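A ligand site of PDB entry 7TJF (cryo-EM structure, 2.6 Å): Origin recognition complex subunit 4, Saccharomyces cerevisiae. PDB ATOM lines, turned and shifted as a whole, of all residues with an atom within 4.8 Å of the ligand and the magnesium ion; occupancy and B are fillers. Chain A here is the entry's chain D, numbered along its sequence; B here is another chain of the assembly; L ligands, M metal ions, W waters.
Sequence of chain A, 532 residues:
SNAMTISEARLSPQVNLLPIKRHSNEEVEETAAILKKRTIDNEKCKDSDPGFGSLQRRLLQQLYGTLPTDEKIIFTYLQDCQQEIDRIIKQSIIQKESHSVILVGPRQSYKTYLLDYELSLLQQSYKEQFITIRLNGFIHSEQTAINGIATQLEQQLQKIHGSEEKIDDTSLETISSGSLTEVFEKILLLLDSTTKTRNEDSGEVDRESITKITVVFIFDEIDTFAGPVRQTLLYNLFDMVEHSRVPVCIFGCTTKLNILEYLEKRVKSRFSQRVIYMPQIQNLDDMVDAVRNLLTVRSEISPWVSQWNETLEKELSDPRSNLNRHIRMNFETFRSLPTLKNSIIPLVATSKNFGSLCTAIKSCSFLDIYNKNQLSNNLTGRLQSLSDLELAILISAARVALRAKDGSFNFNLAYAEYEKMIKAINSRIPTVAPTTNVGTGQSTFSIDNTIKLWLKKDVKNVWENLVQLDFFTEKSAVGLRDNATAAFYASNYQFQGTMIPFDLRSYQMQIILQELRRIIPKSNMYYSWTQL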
ATOM      1  N   TYR A  64      -2.887 -30.443  24.766  1.00  0.00           N
ATOM      2  CA  TYR A  64      -1.850 -29.470  25.081  1.00  0.00           C
ATOM      3  C   TYR A  64      -0.999 -29.082  23.874  1.00  0.00           C
ATOM      4  O   TYR A  64      -0.174 -28.167  23.993  1.00  0.00           O
ATOM      5  CB  TYR A  64      -0.935 -30.008  26.189  1.00  0.00           C
ATOM      6  CG  TYR A  64      -1.513 -29.882  27.582  1.00  0.00           C
ATOM      7  CD1 TYR A  64      -1.595 -28.647  28.214  1.00  0.00           C
ATOM      8  CD2 TYR A  64      -1.969 -30.998  28.259  1.00  0.00           C
ATOM      9  CE1 TYR A  64      -2.123 -28.540  29.485  1.00  0.00           C
ATOM     10  CE2 TYR A  64      -2.503 -30.903  29.524  1.00  0.00           C
ATOM     11  CZ  TYR A  64      -2.576 -29.671  30.135  1.00  0.00           C
ATOM     12  OH  TYR A  64      -3.103 -29.569  31.397  1.00  0.00           O
ATOM     13  N   GLY A  65      -1.182 -29.744  22.731  1.00  0.00           N
ATOM     14  CA  GLY A  65      -0.427 -29.401  21.540  1.00  0.00           C
ATOM     15  C   GLY A  65       1.022 -29.825  21.578  1.00  0.00           C
ATOM     16  O   GLY A  65       1.837 -29.280  20.821  1.00  0.00           O
ATOM     17  N   LYS A  72       1.476 -32.428  14.321  1.00  0.00           N
ATOM     18  CA  LYS A  72       0.867 -31.271  14.968  1.00  0.00           C
ATOM     19  C   LYS A  72      -0.445 -30.899  14.282  1.00  0.00           C
ATOM     20  O   LYS A  72      -0.570 -30.959  13.059  1.00  0.00           O
ATOM     21  CB  LYS A  72       1.824 -30.088  14.960  1.00  0.00           C
ATOM     22  CG  LYS A  72       2.559 -29.905  16.278  1.00  0.00           C
ATOM     23  CD  LYS A  72       2.460 -28.485  16.792  1.00  0.00           C
ATOM     24  CE  LYS A  72       3.476 -28.220  17.896  1.00  0.00           C
ATOM     25  NZ  LYS A  72       3.625 -29.397  18.805  1.00  0.00           N
ATOM     26  N   PRO A 106      -6.156 -11.151  19.227  1.00  0.00           N
ATOM     27  CA  PRO A 106      -6.333 -11.182  20.690  1.00  0.00           C
ATOM     28  C   PRO A 106      -5.433 -12.203  21.367  1.00  0.00           C
ATOM     29  O   PRO A 106      -4.678 -12.915  20.714  1.00  0.00           O
ATOM     30  CB  PRO A 106      -7.810 -11.538  20.860  1.00  0.00           C
ATOM     31  CG  PRO A 106      -8.211 -12.154  19.577  1.00  0.00           C
ATOM     32  CD  PRO A 106      -7.390 -11.503  18.519  1.00  0.00           C
ATOM     33  N   ARG A 107      -5.487 -12.269  22.701  1.00  0.00           N
ATOM     34  CA  ARG A 107      -4.759 -13.292  23.420  1.00  0.00           C
ATOM     35  C   ARG A 107      -5.357 -14.668  23.111  1.00  0.00           C
ATOM     36  O   ARG A 107      -6.555 -14.807  22.875  1.00  0.00           O
ATOM     37  CB  ARG A 107      -4.793 -13.034  24.919  1.00  0.00           C
ATOM     38  CG  ARG A 107      -4.263 -11.668  25.318  1.00  0.00           C
ATOM     39  CD  ARG A 107      -3.388 -11.738  26.551  1.00  0.00           C
ATOM     40  NE  ARG A 107      -2.813 -10.448  26.883  1.00  0.00           N
ATOM     41  CZ  ARG A 107      -1.678  -9.968  26.379  1.00  0.00           C
ATOM     42  NH1 ARG A 107      -0.955 -10.681  25.527  1.00  0.00           N
ATOM     43  NH2 ARG A 107      -1.260  -8.765  26.732  1.00  0.00           N
ATOM     44  N   GLN A 108      -4.472 -15.674  23.087  1.00  0.00           N
ATOM     45  CA  GLN A 108      -4.790 -17.069  22.759  1.00  0.00           C
ATOM     46  C   GLN A 108      -5.419 -17.200  21.364  1.00  0.00           C
ATOM     47  O   GLN A 108      -6.310 -18.022  21.141  1.00  0.00           O
ATOM     48  CB  GLN A 108      -5.690 -17.715  23.818  1.00  0.00           C
ATOM     49  CG  GLN A 108      -5.176 -17.575  25.242  1.00  0.00           C
ATOM     50  CD  GLN A 108      -4.028 -18.530  25.537  1.00  0.00           C
ATOM     51  OE1 GLN A 108      -4.238 -19.680  25.900  1.00  0.00           O
ATOM     52  NE2 GLN A 108      -2.812 -18.042  25.383  1.00  0.00           N
ATOM     53  N   SER A 109      -4.945 -16.388  20.423  1.00  0.00           N
ATOM     54  CA  SER A 109      -5.373 -16.466  19.030  1.00  0.00           C
ATOM     55  C   SER A 109      -4.320 -17.109  18.137  1.00  0.00           C
ATOM     56  O   SER A 109      -4.291 -16.837  16.938  1.00  0.00           O
ATOM     57  CB  SER A 109      -5.757 -15.086  18.502  1.00  0.00           C
ATOM     58  OG  SER A 109      -4.727 -14.146  18.730  1.00  0.00           O
ATOM     59  N   TYR A 110      -3.421 -17.913  18.738  1.00  0.00           N
ATOM     60  CA  TYR A 110      -2.485 -18.803  18.053  1.00  0.00           C
ATOM     61  C   TYR A 110      -1.408 -18.061  17.258  1.00  0.00           C
ATOM     62  O   TYR A 110      -0.952 -18.548  16.229  1.00  0.00           O
ATOM     63  CB  TYR A 110      -3.212 -19.811  17.144  1.00  0.00           C
ATOM     64  CG  TYR A 110      -4.172 -20.723  17.887  1.00  0.00           C
ATOM     65  CD1 TYR A 110      -5.495 -20.348  18.108  1.00  0.00           C
ATOM     66  CD2 TYR A 110      -3.736 -21.944  18.388  1.00  0.00           C
ATOM     67  CE1 TYR A 110      -6.361 -21.170  18.798  1.00  0.00           C
ATOM     68  CE2 TYR A 110      -4.601 -22.772  19.069  1.00  0.00           C
ATOM     69  CZ  TYR A 110      -5.903 -22.381  19.273  1.00  0.00           C
ATOM     70  OH  TYR A 110      -6.769 -23.203  19.962  1.00  0.00           O
ATOM     71  N   LYS A 111      -0.979 -16.886  17.732  1.00  0.00           N
ATOM     72  CA  LYS A 111       0.154 -16.225  17.102  1.00  0.00           C
ATOM     73  C   LYS A 111       1.458 -16.948  17.432  1.00  0.00           C
ATOM     74  O   LYS A 111       2.226 -17.331  16.525  1.00  0.00           O
ATOM     75  CB  LYS A 111       0.225 -14.766  17.554  1.00  0.00           C
ATOM     76  CG  LYS A 111      -1.062 -13.999  17.385  1.00  0.00           C
ATOM     77  CD  LYS A 111      -0.867 -12.496  17.559  1.00  0.00           C
ATOM     78  CE  LYS A 111      -0.575 -12.122  19.014  1.00  0.00           C
ATOM     79  NZ  LYS A 111      -1.725 -12.327  19.914  1.00  0.00           N
ATOM     80  N   THR A 112       1.703 -17.168  18.722  1.00  0.00           N
ATOM     81  CA  THR A 112       2.913 -17.859  19.174  1.00  0.00           C
ATOM     82  C   THR A 112       2.905 -19.319  18.729  1.00  0.00           C
ATOM     83  O   THR A 112       3.959 -19.856  18.352  1.00  0.00           O
ATOM     84  CB  THR A 112       3.032 -17.729  20.691  1.00  0.00           C
ATOM     85  OG1 THR A 112       3.150 -16.349  21.042  1.00  0.00           O
ATOM     86  CG2 THR A 112       4.234 -18.478  21.256  1.00  0.00           C
ATOM     87  N   TYR A 113       1.731 -19.951  18.727  1.00  0.00           N
ATOM     88  CA  TYR A 113       1.603 -21.342  18.301  1.00  0.00           C
ATOM     89  C   TYR A 113       1.982 -21.513  16.833  1.00  0.00           C
ATOM     90  O   TYR A 113       2.766 -22.397  16.476  1.00  0.00           O
ATOM     91  CB  TYR A 113       0.168 -21.824  18.546  1.00  0.00           C
ATOM     92  CG  TYR A 113      -0.148 -23.206  18.026  1.00  0.00           C
ATOM     93  CD1 TYR A 113       0.205 -24.340  18.759  1.00  0.00           C
ATOM     94  CD2 TYR A 113      -0.826 -23.377  16.823  1.00  0.00           C
ATOM     95  CE1 TYR A 113      -0.089 -25.603  18.290  1.00  0.00           C
ATOM     96  CE2 TYR A 113      -1.120 -24.639  16.353  1.00  0.00           C
ATOM     97  CZ  TYR A 113      -0.755 -25.743  17.082  1.00  0.00           C
ATOM     98  OH  TYR A 113      -1.048 -27.006  16.612  1.00  0.00           O
ATOM     99  N   ASP A 116       5.777 -20.739  16.346  1.00  0.00           N
ATOM    100  CA  ASP A 116       6.586 -21.839  16.850  1.00  0.00           C
ATOM    101  C   ASP A 116       6.510 -23.050  15.936  1.00  0.00           C
ATOM    102  O   ASP A 116       7.518 -23.734  15.719  1.00  0.00           O
ATOM    103  CB  ASP A 116       6.143 -22.210  18.261  1.00  0.00           C
ATOM    104  CG  ASP A 116       6.623 -21.232  19.312  1.00  0.00           C
ATOM    105  OD1 ASP A 116       7.205 -20.187  18.942  1.00  0.00           O
ATOM    106  OD2 ASP A 116       6.438 -21.512  20.512  1.00  0.00           O
ATOM    107  N   ASP A 220       7.391 -10.365  20.943  1.00  0.00           N
ATOM    108  CA  ASP A 220       6.098 -10.432  21.614  1.00  0.00           C
ATOM    109  C   ASP A 220       5.835  -9.123  22.336  1.00  0.00           C
ATOM    110  O   ASP A 220       6.757  -8.544  22.930  1.00  0.00           O
ATOM    111  CB  ASP A 220       6.057 -11.593  22.599  1.00  0.00           C
ATOM    112  CG  ASP A 220       6.116 -12.948  21.917  1.00  0.00           C
ATOM    113  OD1 ASP A 220       5.715 -13.043  20.733  1.00  0.00           O
ATOM    114  OD2 ASP A 220       6.558 -13.914  22.564  1.00  0.00           O
ATOM    115  N   GLU A 221       4.582  -8.669  22.301  1.00  0.00           N
ATOM    116  CA  GLU A 221       4.110  -7.412  22.882  1.00  0.00           C
ATOM    117  C   GLU A 221       4.914  -6.215  22.355  1.00  0.00           C
ATOM    118  O   GLU A 221       5.521  -5.454  23.115  1.00  0.00           O
ATOM    119  CB  GLU A 221       4.129  -7.456  24.419  1.00  0.00           C
ATOM    120  CG  GLU A 221       3.607  -8.746  25.025  1.00  0.00           C
ATOM    121  CD  GLU A 221       2.096  -8.847  25.002  1.00  0.00           C
ATOM    122  OE1 GLU A 221       1.433  -7.794  24.930  1.00  0.00           O
ATOM    123  OE2 GLU A 221       1.565  -9.973  25.054  1.00  0.00           O
ATOM    124  N   THR A 255      -1.786  -7.259  20.448  1.00  0.00           N
ATOM    125  CA  THR A 255      -3.234  -7.310  20.506  1.00  0.00           C
ATOM    126  C   THR A 255      -3.889  -6.029  20.018  1.00  0.00           C
ATOM    127  O   THR A 255      -5.090  -6.036  19.742  1.00  0.00           O
ATOM    128  CB  THR A 255      -3.714  -7.605  21.939  1.00  0.00           C
ATOM    129  OG1 THR A 255      -3.236  -6.582  22.827  1.00  0.00           O
ATOM    130  CG2 THR A 255      -3.208  -8.956  22.406  1.00  0.00           C
ATOM    131  N   PRO A 338      -9.162 -22.332  23.521  1.00  0.00           N
ATOM    132  CA  PRO A 338      -8.439 -22.628  24.773  1.00  0.00           C
ATOM    133  C   PRO A 338      -9.301 -22.672  26.027  1.00  0.00           C
ATOM    134  O   PRO A 338      -9.015 -23.464  26.940  1.00  0.00           O
ATOM    135  CB  PRO A 338      -7.405 -21.493  24.858  1.00  0.00           C
ATOM    136  CG  PRO A 338      -7.137 -21.158  23.474  1.00  0.00           C
ATOM    137  CD  PRO A 338      -8.449 -21.267  22.772  1.00  0.00           C
ATOM    138  N   LYS A 341     -10.715 -26.065  25.923  1.00  0.00           N
ATOM    139  CA  LYS A 341      -9.692 -27.055  26.226  1.00  0.00           C
ATOM    140  C   LYS A 341      -9.419 -27.136  27.716  1.00  0.00           C
ATOM    141  O   LYS A 341      -9.173 -28.226  28.251  1.00  0.00           O
ATOM    142  CB  LYS A 341      -8.388 -26.740  25.474  1.00  0.00           C
ATOM    143  CG  LYS A 341      -8.453 -26.926  23.982  1.00  0.00           C
ATOM    144  CD  LYS A 341      -7.057 -26.943  23.381  1.00  0.00           C
ATOM    145  CE  LYS A 341      -6.529 -25.542  23.184  1.00  0.00           C
ATOM    146  NZ  LYS A 341      -5.061 -25.477  23.420  1.00  0.00           N
ATOM    147  N   LYS B 151       4.546 -15.241  30.835  1.00  0.00           N
ATOM    148  CA  LYS B 151       5.318 -15.406  29.610  1.00  0.00           C
ATOM    149  C   LYS B 151       6.760 -15.806  29.875  1.00  0.00           C
ATOM    150  O   LYS B 151       7.570 -15.752  28.945  1.00  0.00           O
ATOM    151  CB  LYS B 151       5.275 -14.112  28.795  1.00  0.00           C
ATOM    152  CG  LYS B 151       3.899 -13.755  28.261  1.00  0.00           C
ATOM    153  CD  LYS B 151       3.306 -14.875  27.428  1.00  0.00           C
ATOM    154  CE  LYS B 151       1.943 -14.492  26.881  1.00  0.00           C
ATOM    155  NZ  LYS B 151       1.242 -15.665  26.310  1.00  0.00           N
ATOM    156  N   GLU B 154       8.186 -18.888  27.883  1.00  0.00           N
ATOM    157  CA  GLU B 154       8.423 -18.738  26.450  1.00  0.00           C
ATOM    158  C   GLU B 154       9.869 -18.367  26.153  1.00  0.00           C
ATOM    159  O   GLU B 154      10.362 -18.656  25.052  1.00  0.00           O
ATOM    160  CB  GLU B 154       7.479 -17.677  25.862  1.00  0.00           C
ATOM    161  CG  GLU B 154       6.012 -17.913  26.184  1.00  0.00           C
ATOM    162  CD  GLU B 154       5.080 -17.425  25.090  1.00  0.00           C
ATOM    163  OE1 GLU B 154       5.466 -16.517  24.328  1.00  0.00           O
ATOM    164  OE2 GLU B 154       3.951 -17.956  24.989  1.00  0.00           O
ATOM    165  N   LYS B 158      12.646 -24.822  25.012  1.00  0.00           N
ATOM    166  CA  LYS B 158      11.541 -25.784  25.053  1.00  0.00           C
ATOM    167  C   LYS B 158      12.031 -27.219  25.116  1.00  0.00           C
ATOM    168  O   LYS B 158      11.333 -28.086  25.652  1.00  0.00           O
ATOM    169  CB  LYS B 158      10.639 -25.578  23.833  1.00  0.00           C
ATOM    170  CG  LYS B 158      11.368 -25.008  22.628  1.00  0.00           C
ATOM    171  CD  LYS B 158      10.420 -24.794  21.456  1.00  0.00           C
ATOM    172  CE  LYS B 158       9.482 -23.629  21.708  1.00  0.00           C
ATOM    173  NZ  LYS B 158       9.268 -22.817  20.480  1.00  0.00           N
ATOM    174  N   HIS B 182      -5.982 -14.691  29.240  1.00  0.00           N
ATOM    175  CA  HIS B 182      -4.826 -15.574  29.103  1.00  0.00           C
ATOM    176  C   HIS B 182      -5.211 -17.043  29.110  1.00  0.00           C
ATOM    177  O   HIS B 182      -4.386 -17.871  28.703  1.00  0.00           O
ATOM    178  CB  HIS B 182      -3.819 -15.282  30.214  1.00  0.00           C
ATOM    179  CG  HIS B 182      -3.051 -14.020  30.004  1.00  0.00           C
ATOM    180  ND1 HIS B 182      -3.370 -12.842  30.645  1.00  0.00           N
ATOM    181  CD2 HIS B 182      -1.978 -13.741  29.227  1.00  0.00           C
ATOM    182  CE1 HIS B 182      -2.531 -11.890  30.271  1.00  0.00           C
ATOM    183  NE2 HIS B 182      -1.675 -12.414  29.407  1.00  0.00           N
HETATM  184  P1  LIG L   1      -0.741 -13.863  23.483  1.00  0.00           P
HETATM  185  O1  LIG L   1      -1.360 -13.807  24.831  1.00  0.00           O
HETATM  186  O2  LIG L   1      -1.155 -12.726  22.559  1.00  0.00           O
HETATM  187  O3  LIG L   1       0.769 -13.920  23.515  1.00  0.00           O
HETATM  188  P2  LIG L   1      -1.180 -15.794  21.268  1.00  0.00           P
HETATM  189  O4  LIG L   1      -2.098 -15.085  20.362  1.00  0.00           O
HETATM  190  O5  LIG L   1       0.269 -15.856  20.812  1.00  0.00           O
HETATM  191  O6  LIG L   1      -1.184 -15.191  22.713  1.00  0.00           O
HETATM  192  P3  LIG L   1      -0.985 -18.673  21.932  1.00  0.00           P
HETATM  193  O7  LIG L   1      -0.392 -19.348  20.758  1.00  0.00           O
HETATM  194  O8  LIG L   1      -0.008 -18.386  23.065  1.00  0.00           O
HETATM  195  O9  LIG L   1      -1.654 -17.291  21.535  1.00  0.00           O
HETATM  196  O10 LIG L   1      -2.203 -19.477  22.518  1.00  0.00           O
HETATM  197  C1  LIG L   1      -3.034 -20.316  21.688  1.00  0.00           C
HETATM  198  C2  LIG L   1      -2.984 -21.744  22.165  1.00  0.00           C
HETATM  199  O11 LIG L   1      -1.800 -22.396  21.659  1.00  0.00           O
HETATM  200  C3  LIG L   1      -2.990 -21.969  23.674  1.00  0.00           C
HETATM  201  O12 LIG L   1      -3.869 -23.034  24.038  1.00  0.00           O
HETATM  202  C4  LIG L   1      -1.526 -22.320  23.994  1.00  0.00           C
HETATM  203  O13 LIG L   1      -1.413 -23.205  25.104  1.00  0.00           O
HETATM  204  C5  LIG L   1      -1.102 -23.029  22.707  1.00  0.00           C
HETATM  205  N1  LIG L   1       0.325 -22.929  22.423  1.00  0.00           N
HETATM  206  C6  LIG L   1       1.063 -21.777  22.296  1.00  0.00           C
HETATM  207  N2  LIG L   1       2.338 -21.990  22.035  1.00  0.00           N
HETATM  208  C7  LIG L   1       2.439 -23.374  21.985  1.00  0.00           C
HETATM  209  C8  LIG L   1       3.514 -24.237  21.749  1.00  0.00           C
HETATM  210  N3  LIG L   1       4.763 -23.825  21.501  1.00  0.00           N
HETATM  211  N4  LIG L   1       3.280 -25.571  21.763  1.00  0.00           N
HETATM  212  C9  LIG L   1       2.033 -26.000  22.009  1.00  0.00           C
HETATM  213  N5  LIG L   1       0.935 -25.274  22.251  1.00  0.00           N
HETATM  214  C10 LIG L   1       1.200 -23.965  22.219  1.00  0.00           C
HETATM  215 MG    MG M   1       2.016 -15.192  22.386  1.00  0.00          MG
HETATM  216  O   HOH W   1       1.654 -16.828  23.642  1.00  0.00           O
HETATM  217  O   HOH W   2       3.823 -14.635  23.379  1.00  0.00           O
HETATM  218  O   HOH W   3       2.587 -12.117  24.533  1.00  0.00           O
HETATM  219  O   HOH W   4       2.057 -13.717  20.866  1.00  0.00           O
HETATM  220  O   HOH W   5      -0.007 -19.809  25.643  1.00  0.00           O
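The backbone carbonyl oxygen (O) of Pro 106 sits at hydrogen-bond distance from the side-chain amino group (NZ) of Lys 111 (3.1 Å). The side-chain carboxylate (OD2) of Asp 116 is in salt-bridge range of the side-chain amino group (NZ) of Lys 158 of chain B. The guanidinium group of Arg 107 is in salt-bridge range of the side-chain carboxylate of Glu 221 (2.7 Å). NE2 of His 182 of chain B sits at hydrogen-bond distance from NE of Arg 107 (3.4 Å). OE1 of Gln 108 sits close to O of His 182 of chain B. NZ of Lys 151 of chain B lies within salt-bridge range of OE2 of Glu 154 of chain B (3.8 Å). The side-chain amino group (NZ) of Lys 72 lies within hydrogen-bond range of the backbone carbonyl oxygen (O) of Gly 65 (2.7 Å).
Water W1 lies within hydrogen-bond range of OE2 of Glu 154 of chain B (2.9 Å), NZ of Lys 151 of chain B (2.9 Å) and O6 of the ligand (3.4 Å). Water W2 lies within hydrogen-bond range of the side-chain carboxylate of Glu 154 of chain B (2.7 Å) and the side-chain carboxylate of Asp 220 (2.9 Å). Water W5 bridges O8 of the ligand (2.9 Å) and NE2 of Gln 108 (3.3 Å).
An oxygen (O5) of the ligand lies close to the backbone NH (N) of Thr 112 (2.9 Å). An oxygen (O4) of the ligand sits close to the backbone NH of Lys 111, at 3.4 Å. The side-chain amino group of Lys 111 lies within salt-bridge range of an oxygen (O2) of the ligand (2.7 Å). O12 of the ligand sits at hydrogen-bond distance from NZ of Lys 341, 2.8 Å away. An oxygen (O7) of the ligand sits at hydrogen-bond distance from the backbone NH (N) of Tyr 113, at 3.0 Å. A nitrogen (N3) of the ligand is in hydrogen-bond range of the side-chain carboxylate of Asp 116, at 3.0 Å. O4 of the ligand is in hydrogen-bond range of N of Ser 109 (3.1 Å). OG of Ser 109 sits at hydrogen-bond distance from O4 of the ligand (3.2 Å). The guanidinium group (NH1) of Arg 107 is in salt-bridge range of an oxygen (O1) of the ligand. O6 of the ligand is in hydrogen-bond range of N of Gln 108, 3.3 Å away. O10 of the ligand lies within hydrogen-bond range of NE2 of Gln 108. The side-chain amino group (NZ) of Lys 151 of chain B is in salt-bridge range of an oxygen (O1) of the ligand, at 3.5 Å. The backbone NH (N) of Tyr 110 sits at hydrogen-bond distance from an oxygen (O9) of the ligand (3.4 Å).
The magnesium ion is bound by water W1 (2.1 Å), OG1 of Thr 112 (2.1 Å), O3 of the ligand (2.1 Å), water W4 (2.1 Å), water W2 (2.1 Å) and O5 of the ligand (2.4 Å). The magnesium ion has six donor atoms within binding distance.
An oxygen (O4) of the ligand sits close to the backbone carbonyl oxygen (O) of Pro 106 (3.4 Å). O of Tyr 64 touches N5 of the ligand, 3.6 Å away. Gly 65 touches the ligand (O to C9, 3.5 Å). Pro 338 touches the ligand (CG to O12, 3.8 Å). Hydrophobic or aromatic side chains that line the ligand: Tyr 110, Tyr 113 and Pro 338. Of the 21 residues printed, 14 come within 4 Å of the ligand. Along chain A the residues within 4 Å of the ligand span positions 64 to 341.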
